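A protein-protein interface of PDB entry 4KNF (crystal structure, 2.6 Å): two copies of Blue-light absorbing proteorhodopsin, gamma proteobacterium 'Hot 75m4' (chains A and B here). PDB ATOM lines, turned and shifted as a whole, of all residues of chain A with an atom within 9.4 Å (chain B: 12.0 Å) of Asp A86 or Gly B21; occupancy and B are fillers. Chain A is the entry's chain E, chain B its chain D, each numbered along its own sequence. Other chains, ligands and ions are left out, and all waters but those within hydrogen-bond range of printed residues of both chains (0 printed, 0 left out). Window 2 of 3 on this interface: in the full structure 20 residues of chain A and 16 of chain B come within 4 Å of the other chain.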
ATOM      1  N   ASP A  28     -38.990 -30.292 -13.914  1.00  0.00           N
ATOM      2  CA  ASP A  28     -37.806 -29.446 -13.883  1.00  0.00           C
ATOM      3  C   ASP A  28     -37.505 -28.950 -15.310  1.00  0.00           C
ATOM      4  O   ASP A  28     -36.614 -29.455 -15.996  1.00  0.00           O
ATOM      5  CB  ASP A  28     -36.630 -30.186 -13.243  1.00  0.00           C
ATOM      6  CG  ASP A  28     -35.398 -29.308 -13.080  1.00  0.00           C
ATOM      7  OD1 ASP A  28     -35.348 -28.192 -13.672  1.00  0.00           O
ATOM      8  OD2 ASP A  28     -34.463 -29.742 -12.369  1.00  0.00           O
ATOM      9  N   GLY A  31     -33.908 -28.177 -15.887  1.00  0.00           N
ATOM     10  CA  GLY A  31     -33.283 -29.504 -15.954  1.00  0.00           C
ATOM     11  C   GLY A  31     -33.320 -30.068 -17.379  1.00  0.00           C
ATOM     12  O   GLY A  31     -32.288 -30.393 -17.944  1.00  0.00           O
ATOM     13  N   LEU A  78     -22.478 -30.171 -19.383  1.00  0.00           N
ATOM     14  CA  LEU A  78     -22.568 -31.356 -18.605  1.00  0.00           C
ATOM     15  C   LEU A  78     -22.379 -30.937 -17.126  1.00  0.00           C
ATOM     16  O   LEU A  78     -23.175 -31.308 -16.274  1.00  0.00           O
ATOM     17  CB  LEU A  78     -21.477 -32.310 -19.069  1.00  0.00           C
ATOM     18  CG  LEU A  78     -21.672 -33.820 -19.078  1.00  0.00           C
ATOM     19  CD1 LEU A  78     -22.969 -34.192 -19.777  1.00  0.00           C
ATOM     20  CD2 LEU A  78     -20.470 -34.492 -19.752  1.00  0.00           C
ATOM     21  N   TYR A  79     -21.348 -30.137 -16.840  1.00  0.00           N
ATOM     22  CA  TYR A  79     -21.158 -29.585 -15.504  1.00  0.00           C
ATOM     23  C   TYR A  79     -22.292 -28.668 -15.084  1.00  0.00           C
ATOM     24  O   TYR A  79     -22.711 -28.684 -13.919  1.00  0.00           O
ATOM     25  CB  TYR A  79     -19.818 -28.875 -15.377  1.00  0.00           C
ATOM     26  CG  TYR A  79     -18.697 -29.865 -15.286  1.00  0.00           C
ATOM     27  CD1 TYR A  79     -18.379 -30.462 -14.065  1.00  0.00           C
ATOM     28  CD2 TYR A  79     -17.988 -30.259 -16.425  1.00  0.00           C
ATOM     29  CE1 TYR A  79     -17.378 -31.405 -13.971  1.00  0.00           C
ATOM     30  CE2 TYR A  79     -16.982 -31.204 -16.341  1.00  0.00           C
ATOM     31  CZ  TYR A  79     -16.681 -31.769 -15.108  1.00  0.00           C
ATOM     32  OH  TYR A  79     -15.675 -32.691 -15.000  1.00  0.00           O
ATOM     33  N   MET A  80     -22.810 -27.885 -16.025  1.00  0.00           N
ATOM     34  CA  MET A  80     -23.896 -26.964 -15.674  1.00  0.00           C
ATOM     35  C   MET A  80     -25.157 -27.689 -15.231  1.00  0.00           C
ATOM     36  O   MET A  80     -25.855 -27.203 -14.348  1.00  0.00           O
ATOM     37  CB  MET A  80     -24.209 -25.955 -16.785  1.00  0.00           C
ATOM     38  CG  MET A  80     -23.292 -24.743 -16.765  1.00  0.00           C
ATOM     39  SD  MET A  80     -23.581 -23.543 -18.094  1.00  0.00           S
ATOM     40  CE  MET A  80     -23.565 -24.487 -19.597  1.00  0.00           C
ATOM     41  N   ARG A  81     -25.446 -28.841 -15.834  1.00  0.00           N
ATOM     42  CA  ARG A  81     -26.662 -29.556 -15.501  1.00  0.00           C
ATOM     43  C   ARG A  81     -26.499 -30.262 -14.135  1.00  0.00           C
ATOM     44  O   ARG A  81     -27.418 -30.298 -13.316  1.00  0.00           O
ATOM     45  CB  ARG A  81     -27.010 -30.534 -16.592  1.00  0.00           C
ATOM     46  CG  ARG A  81     -28.450 -30.963 -16.508  1.00  0.00           C
ATOM     47  CD  ARG A  81     -28.754 -32.181 -17.367  1.00  0.00           C
ATOM     48  NE  ARG A  81     -30.186 -32.481 -17.297  1.00  0.00           N
ATOM     49  CZ  ARG A  81     -30.746 -33.331 -16.434  1.00  0.00           C
ATOM     50  NH1 ARG A  81     -30.006 -34.015 -15.566  1.00  0.00           N
ATOM     51  NH2 ARG A  81     -32.060 -33.505 -16.448  1.00  0.00           N
ATOM     52  N   GLY A  82     -25.297 -30.783 -13.903  1.00  0.00           N
ATOM     53  CA  GLY A  82     -24.937 -31.401 -12.649  1.00  0.00           C
ATOM     54  C   GLY A  82     -25.228 -30.435 -11.535  1.00  0.00           C
ATOM     55  O   GLY A  82     -25.884 -30.797 -10.569  1.00  0.00           O
ATOM     56  N   VAL A  83     -24.749 -29.197 -11.692  1.00  0.00           N
ATOM     57  CA  VAL A  83     -24.976 -28.136 -10.705  1.00  0.00           C
ATOM     58  C   VAL A  83     -26.466 -27.793 -10.516  1.00  0.00           C
ATOM     59  O   VAL A  83     -26.905 -27.527  -9.388  1.00  0.00           O
ATOM     60  CB  VAL A  83     -24.127 -26.886 -10.998  1.00  0.00           C
ATOM     61  CG1 VAL A  83     -24.670 -25.653 -10.263  1.00  0.00           C
ATOM     62  CG2 VAL A  83     -22.676 -27.163 -10.625  1.00  0.00           C
ATOM     63  N   TRP A  84     -27.247 -27.848 -11.588  1.00  0.00           N
ATOM     64  CA  TRP A  84     -28.686 -27.535 -11.477  1.00  0.00           C
ATOM     65  C   TRP A  84     -29.518 -28.601 -10.740  1.00  0.00           C
ATOM     66  O   TRP A  84     -30.543 -28.282 -10.136  1.00  0.00           O
ATOM     67  CB  TRP A  84     -29.289 -27.272 -12.841  1.00  0.00           C
ATOM     68  CG  TRP A  84     -30.689 -26.855 -12.823  1.00  0.00           C
ATOM     69  CD1 TRP A  84     -31.768 -27.599 -13.221  1.00  0.00           C
ATOM     70  CD2 TRP A  84     -31.211 -25.570 -12.423  1.00  0.00           C
ATOM     71  NE1 TRP A  84     -32.944 -26.848 -13.098  1.00  0.00           N
ATOM     72  CE2 TRP A  84     -32.626 -25.606 -12.614  1.00  0.00           C
ATOM     73  CE3 TRP A  84     -30.621 -24.386 -11.927  1.00  0.00           C
ATOM     74  CZ2 TRP A  84     -33.460 -24.512 -12.328  1.00  0.00           C
ATOM     75  CZ3 TRP A  84     -31.448 -23.279 -11.656  1.00  0.00           C
ATOM     76  CH2 TRP A  84     -32.862 -23.359 -11.848  1.00  0.00           C
ATOM     77  N   ILE A  85     -29.081 -29.853 -10.812  1.00  0.00           N
ATOM     78  CA  ILE A  85     -29.774 -30.948 -10.153  1.00  0.00           C
ATOM     79  C   ILE A  85     -29.381 -31.031  -8.675  1.00  0.00           C
ATOM     80  O   ILE A  85     -30.238 -31.011  -7.797  1.00  0.00           O
ATOM     81  CB  ILE A  85     -29.485 -32.309 -10.832  1.00  0.00           C
ATOM     82  CG1 ILE A  85     -29.746 -32.252 -12.347  1.00  0.00           C
ATOM     83  CG2 ILE A  85     -30.279 -33.420 -10.152  1.00  0.00           C
ATOM     84  CD1 ILE A  85     -31.128 -31.800 -12.759  1.00  0.00           C
ATOM     85  N   ASP A  86     -28.079 -31.123  -8.423  1.00  0.00           N
ATOM     86  CA  ASP A  86     -27.532 -31.290  -7.079  1.00  0.00           C
ATOM     87  C   ASP A  86     -27.872 -30.138  -6.135  1.00  0.00           C
ATOM     88  O   ASP A  86     -28.062 -30.352  -4.946  1.00  0.00           O
ATOM     89  CB  ASP A  86     -26.011 -31.483  -7.143  1.00  0.00           C
ATOM     90  CG  ASP A  86     -25.601 -32.745  -7.912  1.00  0.00           C
ATOM     91  OD1 ASP A  86     -26.434 -33.309  -8.662  1.00  0.00           O
ATOM     92  OD2 ASP A  86     -24.430 -33.172  -7.770  1.00  0.00           O
ATOM     93  N   THR A  87     -27.942 -28.921  -6.657  1.00  0.00           N
ATOM     94  CA  THR A  87     -28.145 -27.758  -5.804  1.00  0.00           C
ATOM     95  C   THR A  87     -29.397 -26.957  -6.180  1.00  0.00           C
ATOM     96  O   THR A  87     -29.971 -26.266  -5.342  1.00  0.00           O
ATOM     97  CB  THR A  87     -26.902 -26.831  -5.791  1.00  0.00           C
ATOM     98  OG1 THR A  87     -26.896 -26.001  -6.956  1.00  0.00           O
ATOM     99  CG2 THR A  87     -25.622 -27.637  -5.759  1.00  0.00           C
ATOM    100  N   GLY A  88     -29.813 -27.039  -7.438  1.00  0.00           N
ATOM    101  CA  GLY A  88     -30.905 -26.204  -7.918  1.00  0.00           C
ATOM    102  C   GLY A  88     -30.498 -24.755  -8.120  1.00  0.00           C
ATOM    103  O   GLY A  88     -31.319 -23.941  -8.541  1.00  0.00           O
ATOM    104  N   ASP A  89     -29.238 -24.437  -7.813  1.00  0.00           N
ATOM    105  CA  ASP A  89     -28.673 -23.103  -8.057  1.00  0.00           C
ATOM    106  C   ASP A  89     -28.234 -22.879  -9.505  1.00  0.00           C
ATOM    107  O   ASP A  89     -28.003 -23.824 -10.259  1.00  0.00           O
ATOM    108  CB  ASP A  89     -27.464 -22.843  -7.158  1.00  0.00           C
ATOM    109  CG  ASP A  89     -27.818 -22.813  -5.696  1.00  0.00           C
ATOM    110  OD1 ASP A  89     -28.653 -21.967  -5.293  1.00  0.00           O
ATOM    111  OD2 ASP A  89     -27.235 -23.627  -4.947  1.00  0.00           O
ATOM    112  N   THR A  90     -28.102 -21.610  -9.872  1.00  0.00           N
ATOM    113  CA  THR A  90     -27.584 -21.213 -11.174  1.00  0.00           C
ATOM    114  C   THR A  90     -26.076 -21.410 -11.240  1.00  0.00           C
ATOM    115  O   THR A  90     -25.338 -20.901 -10.392  1.00  0.00           O
ATOM    116  CB  THR A  90     -27.966 -19.763 -11.481  1.00  0.00           C
ATOM    117  OG1 THR A  90     -29.389 -19.684 -11.495  1.00  0.00           O
ATOM    118  CG2 THR A  90     -27.445 -19.316 -12.844  1.00  0.00           C
ATOM    119  N   PRO A  91     -25.613 -22.174 -12.242  1.00  0.00           N
ATOM    120  CA  PRO A  91     -24.175 -22.411 -12.384  1.00  0.00           C
ATOM    121  C   PRO A  91     -23.498 -21.254 -13.128  1.00  0.00           C
ATOM    122  O   PRO A  91     -23.011 -21.421 -14.246  1.00  0.00           O
ATOM    123  CB  PRO A  91     -24.111 -23.726 -13.164  1.00  0.00           C
ATOM    124  CG  PRO A  91     -25.419 -23.834 -13.876  1.00  0.00           C
ATOM    125  CD  PRO A  91     -26.408 -22.877 -13.267  1.00  0.00           C
ATOM    126  N   PHE A  94     -19.595 -21.815 -14.034  1.00  0.00           N
ATOM    127  CA  PHE A  94     -19.455 -22.696 -15.198  1.00  0.00           C
ATOM    128  C   PHE A  94     -19.904 -22.009 -16.509  1.00  0.00           C
ATOM    129  O   PHE A  94     -19.263 -22.170 -17.538  1.00  0.00           O
ATOM    130  CB  PHE A  94     -20.186 -24.029 -15.024  1.00  0.00           C
ATOM    131  CG  PHE A  94     -19.423 -25.046 -14.231  1.00  0.00           C
ATOM    132  CD1 PHE A  94     -18.187 -25.499 -14.666  1.00  0.00           C
ATOM    133  CD2 PHE A  94     -19.959 -25.575 -13.027  1.00  0.00           C
ATOM    134  CE1 PHE A  94     -17.479 -26.435 -13.925  1.00  0.00           C
ATOM    135  CE2 PHE A  94     -19.253 -26.510 -12.278  1.00  0.00           C
ATOM    136  CZ  PHE A  94     -18.010 -26.941 -12.725  1.00  0.00           C
ATOM    137  N   GLY B  21     -20.016 -31.458  -6.619  1.00  0.00           N
ATOM    138  CA  GLY B  21     -21.176 -31.250  -7.537  1.00  0.00           C
ATOM    139  C   GLY B  21     -21.727 -29.831  -7.539  1.00  0.00           C
ATOM    140  O   GLY B  21     -22.780 -29.575  -8.131  1.00  0.00           O
ATOM    141  N   GLY B  22     -21.024 -28.914  -6.870  1.00  0.00           N
ATOM    142  CA  GLY B  22     -21.403 -27.498  -6.850  1.00  0.00           C
ATOM    143  C   GLY B  22     -20.806 -26.734  -8.024  1.00  0.00           C
ATOM    144  O   GLY B  22     -20.136 -27.311  -8.888  1.00  0.00           O
ATOM    145  N   ASP B  23     -21.068 -25.431  -8.069  1.00  0.00           N
ATOM    146  CA  ASP B  23     -20.482 -24.545  -9.071  1.00  0.00           C
ATOM    147  C   ASP B  23     -18.986 -24.380  -8.784  1.00  0.00           C
ATOM    148  O   ASP B  23     -18.546 -24.607  -7.655  1.00  0.00           O
ATOM    149  CB  ASP B  23     -21.190 -23.190  -9.040  1.00  0.00           C
ATOM    150  CG  ASP B  23     -21.076 -22.407 -10.371  1.00  0.00           C
ATOM    151  OD1 ASP B  23     -20.486 -22.931 -11.358  1.00  0.00           O
ATOM    152  OD2 ASP B  23     -21.580 -21.245 -10.414  1.00  0.00           O
ATOM    153  N   LEU B  24     -18.209 -24.021  -9.808  1.00  0.00           N
ATOM    154  CA  LEU B  24     -16.776 -23.747  -9.645  1.00  0.00           C
ATOM    155  C   LEU B  24     -16.550 -22.680  -8.571  1.00  0.00           C
ATOM    156  O   LEU B  24     -17.237 -21.649  -8.544  1.00  0.00           O
ATOM    157  CB  LEU B  24     -16.155 -23.283 -10.969  1.00  0.00           C
ATOM    158  CG  LEU B  24     -15.483 -24.248 -11.947  1.00  0.00           C
ATOM    159  CD1 LEU B  24     -15.360 -23.593 -13.322  1.00  0.00           C
ATOM    160  CD2 LEU B  24     -14.118 -24.652 -11.425  1.00  0.00           C
ATOM    161  N   ASP B  25     -15.599 -22.925  -7.678  1.00  0.00           N
ATOM    162  CA  ASP B  25     -15.321 -21.964  -6.629  1.00  0.00           C
ATOM    163  C   ASP B  25     -14.656 -20.724  -7.238  1.00  0.00           C
ATOM    164  O   ASP B  25     -13.569 -20.807  -7.807  1.00  0.00           O
ATOM    165  CB  ASP B  25     -14.451 -22.596  -5.550  1.00  0.00           C
ATOM    166  CG  ASP B  25     -14.364 -21.752  -4.305  1.00  0.00           C
ATOM    167  OD1 ASP B  25     -15.109 -20.747  -4.195  1.00  0.00           O
ATOM    168  OD2 ASP B  25     -13.543 -22.104  -3.430  1.00  0.00           O
ATOM    169  N   TRP B  35      -8.493 -24.922 -14.564  1.00  0.00           N
ATOM    170  CA  TRP B  35      -9.680 -25.311 -15.289  1.00  0.00           C
ATOM    171  C   TRP B  35      -9.569 -24.802 -16.718  1.00  0.00           C
ATOM    172  O   TRP B  35      -9.678 -25.574 -17.657  1.00  0.00           O
ATOM    173  CB  TRP B  35     -10.941 -24.740 -14.646  1.00  0.00           C
ATOM    174  CG  TRP B  35     -12.125 -25.122 -15.437  1.00  0.00           C
ATOM    175  CD1 TRP B  35     -12.570 -24.528 -16.590  1.00  0.00           C
ATOM    176  CD2 TRP B  35     -12.972 -26.240 -15.207  1.00  0.00           C
ATOM    177  NE1 TRP B  35     -13.644 -25.206 -17.083  1.00  0.00           N
ATOM    178  CE2 TRP B  35     -13.916 -26.266 -16.254  1.00  0.00           C
ATOM    179  CE3 TRP B  35     -13.033 -27.220 -14.213  1.00  0.00           C
ATOM    180  CZ2 TRP B  35     -14.921 -27.238 -16.330  1.00  0.00           C
ATOM    181  CZ3 TRP B  35     -14.026 -28.179 -14.285  1.00  0.00           C
ATOM    182  CH2 TRP B  35     -14.955 -28.187 -15.340  1.00  0.00           C
ATOM    183  N   ARG B  81      -4.957 -30.036 -11.389  1.00  0.00           N
ATOM    184  CA  ARG B  81      -6.127 -29.382 -10.833  1.00  0.00           C
ATOM    185  C   ARG B  81      -6.810 -30.184  -9.700  1.00  0.00           C
ATOM    186  O   ARG B  81      -7.356 -29.591  -8.782  1.00  0.00           O
ATOM    187  CB  ARG B  81      -7.135 -29.026 -11.908  1.00  0.00           C
ATOM    188  CG  ARG B  81      -8.211 -28.095 -11.365  1.00  0.00           C
ATOM    189  CD  ARG B  81      -9.309 -27.810 -12.362  1.00  0.00           C
ATOM    190  NE  ARG B  81     -10.613 -27.986 -11.731  1.00  0.00           N
ATOM    191  CZ  ARG B  81     -11.269 -27.046 -11.057  1.00  0.00           C
ATOM    192  NH1 ARG B  81     -10.760 -25.831 -10.918  1.00  0.00           N
ATOM    193  NH2 ARG B  81     -12.445 -27.328 -10.518  1.00  0.00           N
ATOM    194  N   ILE B  85      -7.420 -28.871  -5.790  1.00  0.00           N
ATOM    195  CA  ILE B  85      -8.722 -28.716  -5.142  1.00  0.00           C
ATOM    196  C   ILE B  85      -8.907 -29.663  -3.961  1.00  0.00           C
ATOM    197  O   ILE B  85      -9.598 -29.331  -3.008  1.00  0.00           O
ATOM    198  CB  ILE B  85      -9.930 -28.809  -6.119  1.00  0.00           C
ATOM    199  CG1 ILE B  85     -10.103 -30.239  -6.644  1.00  0.00           C
ATOM    200  CG2 ILE B  85      -9.829 -27.752  -7.228  1.00  0.00           C
ATOM    201  CD1 ILE B  85     -11.520 -30.576  -7.061  1.00  0.00           C
ATOM    202  N   ASP B  86      -8.287 -30.832  -4.021  1.00  0.00           N
ATOM    203  CA  ASP B  86      -8.491 -31.833  -2.981  1.00  0.00           C
ATOM    204  C   ASP B  86      -7.599 -31.635  -1.757  1.00  0.00           C
ATOM    205  O   ASP B  86      -7.961 -32.050  -0.654  1.00  0.00           O
ATOM    206  CB  ASP B  86      -8.367 -33.254  -3.540  1.00  0.00           C
ATOM    207  CG  ASP B  86      -9.676 -33.766  -4.127  1.00  0.00           C
ATOM    208  OD1 ASP B  86     -10.138 -33.216  -5.153  1.00  0.00           O
ATOM    209  OD2 ASP B  86     -10.250 -34.722  -3.556  1.00  0.00           O
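OD1 of Asp B23 sits at hydrogen-bond distance from N of Phe A94, at 3.0 Å.
The side-chain hydroxyl (OG1) of Thr A87 lies within hydrogen-bond range of the backbone carbonyl oxygen (O) of Val A83 (2.9 Å).
Among the printed residues, merely in contact across the chains: Tyr A79 with Trp B35 (3.8 Å), Val A83 with Gly B21 (3.5 Å), Val A83 with Gly B22 (3.1 Å), Val A83 with Asp B23 (3.5 Å), Asp A86 with Gly B21 (3.8 Å), Thr A90 with Asp B23 (3.8 Å), Pro A91 with Asp B23 (3.3 Å), Phe A94 with Gly B22 (3.6 Å), Phe A94 with Leu B24 (3.6 Å) and Phe A94 with Trp B35 (3.4 Å).
Of chain B, only Gly B21 (3.8 Å) comes within 4 Å of Asp A86. Gly B21 touches just these residues of chain A: Val A83 (3.5 Å) and Asp A86 (3.8 Å). No residue of chain B comes within 4 Å of Gly A82. Printed residues of chain B within 4 Å of Val A83: Gly B21 (3.5 Å), Gly B22 (3.1 Å) and Asp B23 (3.5 Å). No residue of chain B comes within 4 Å of Ile A85. Printed residues of chain B within 4 Å of Tyr A79: Trp B35. Printed residues of chain A within 4 Å of Asp B23: Val A83, Thr A90, Pro A91 and Phe A94. Arg A81 touches none of the printed residues of chain B. Gly A31 touches none of the printed residues of chain B. The nearest residue of chain B that does not touch Asp A86 is Gly B22 (5.5 Å).
Hydrophobic or aromatic side chains of chain A within 4 Å of the printed part of chain B: Tyr A79, Val A83 and Phe A94. Printed residues of chain B that touch a printed residue of chain A: Gly B21, Gly B22, Asp B23, Leu B24 and Trp B35. Hydrophobic or aromatic side chains of chain B within 4 Å of the printed part of chain A: Leu B24 and Trp B35. Among the printed residues, no Asp or Glu carboxylate lies within 4 Å of a Lys or Arg side-chain nitrogen of the other chain.
Positions printed for both chains: 81, 85 and 86. Of the 11 pairs that touch across the chains among the printed residues, none has its exchanged pair printed and touching as well.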
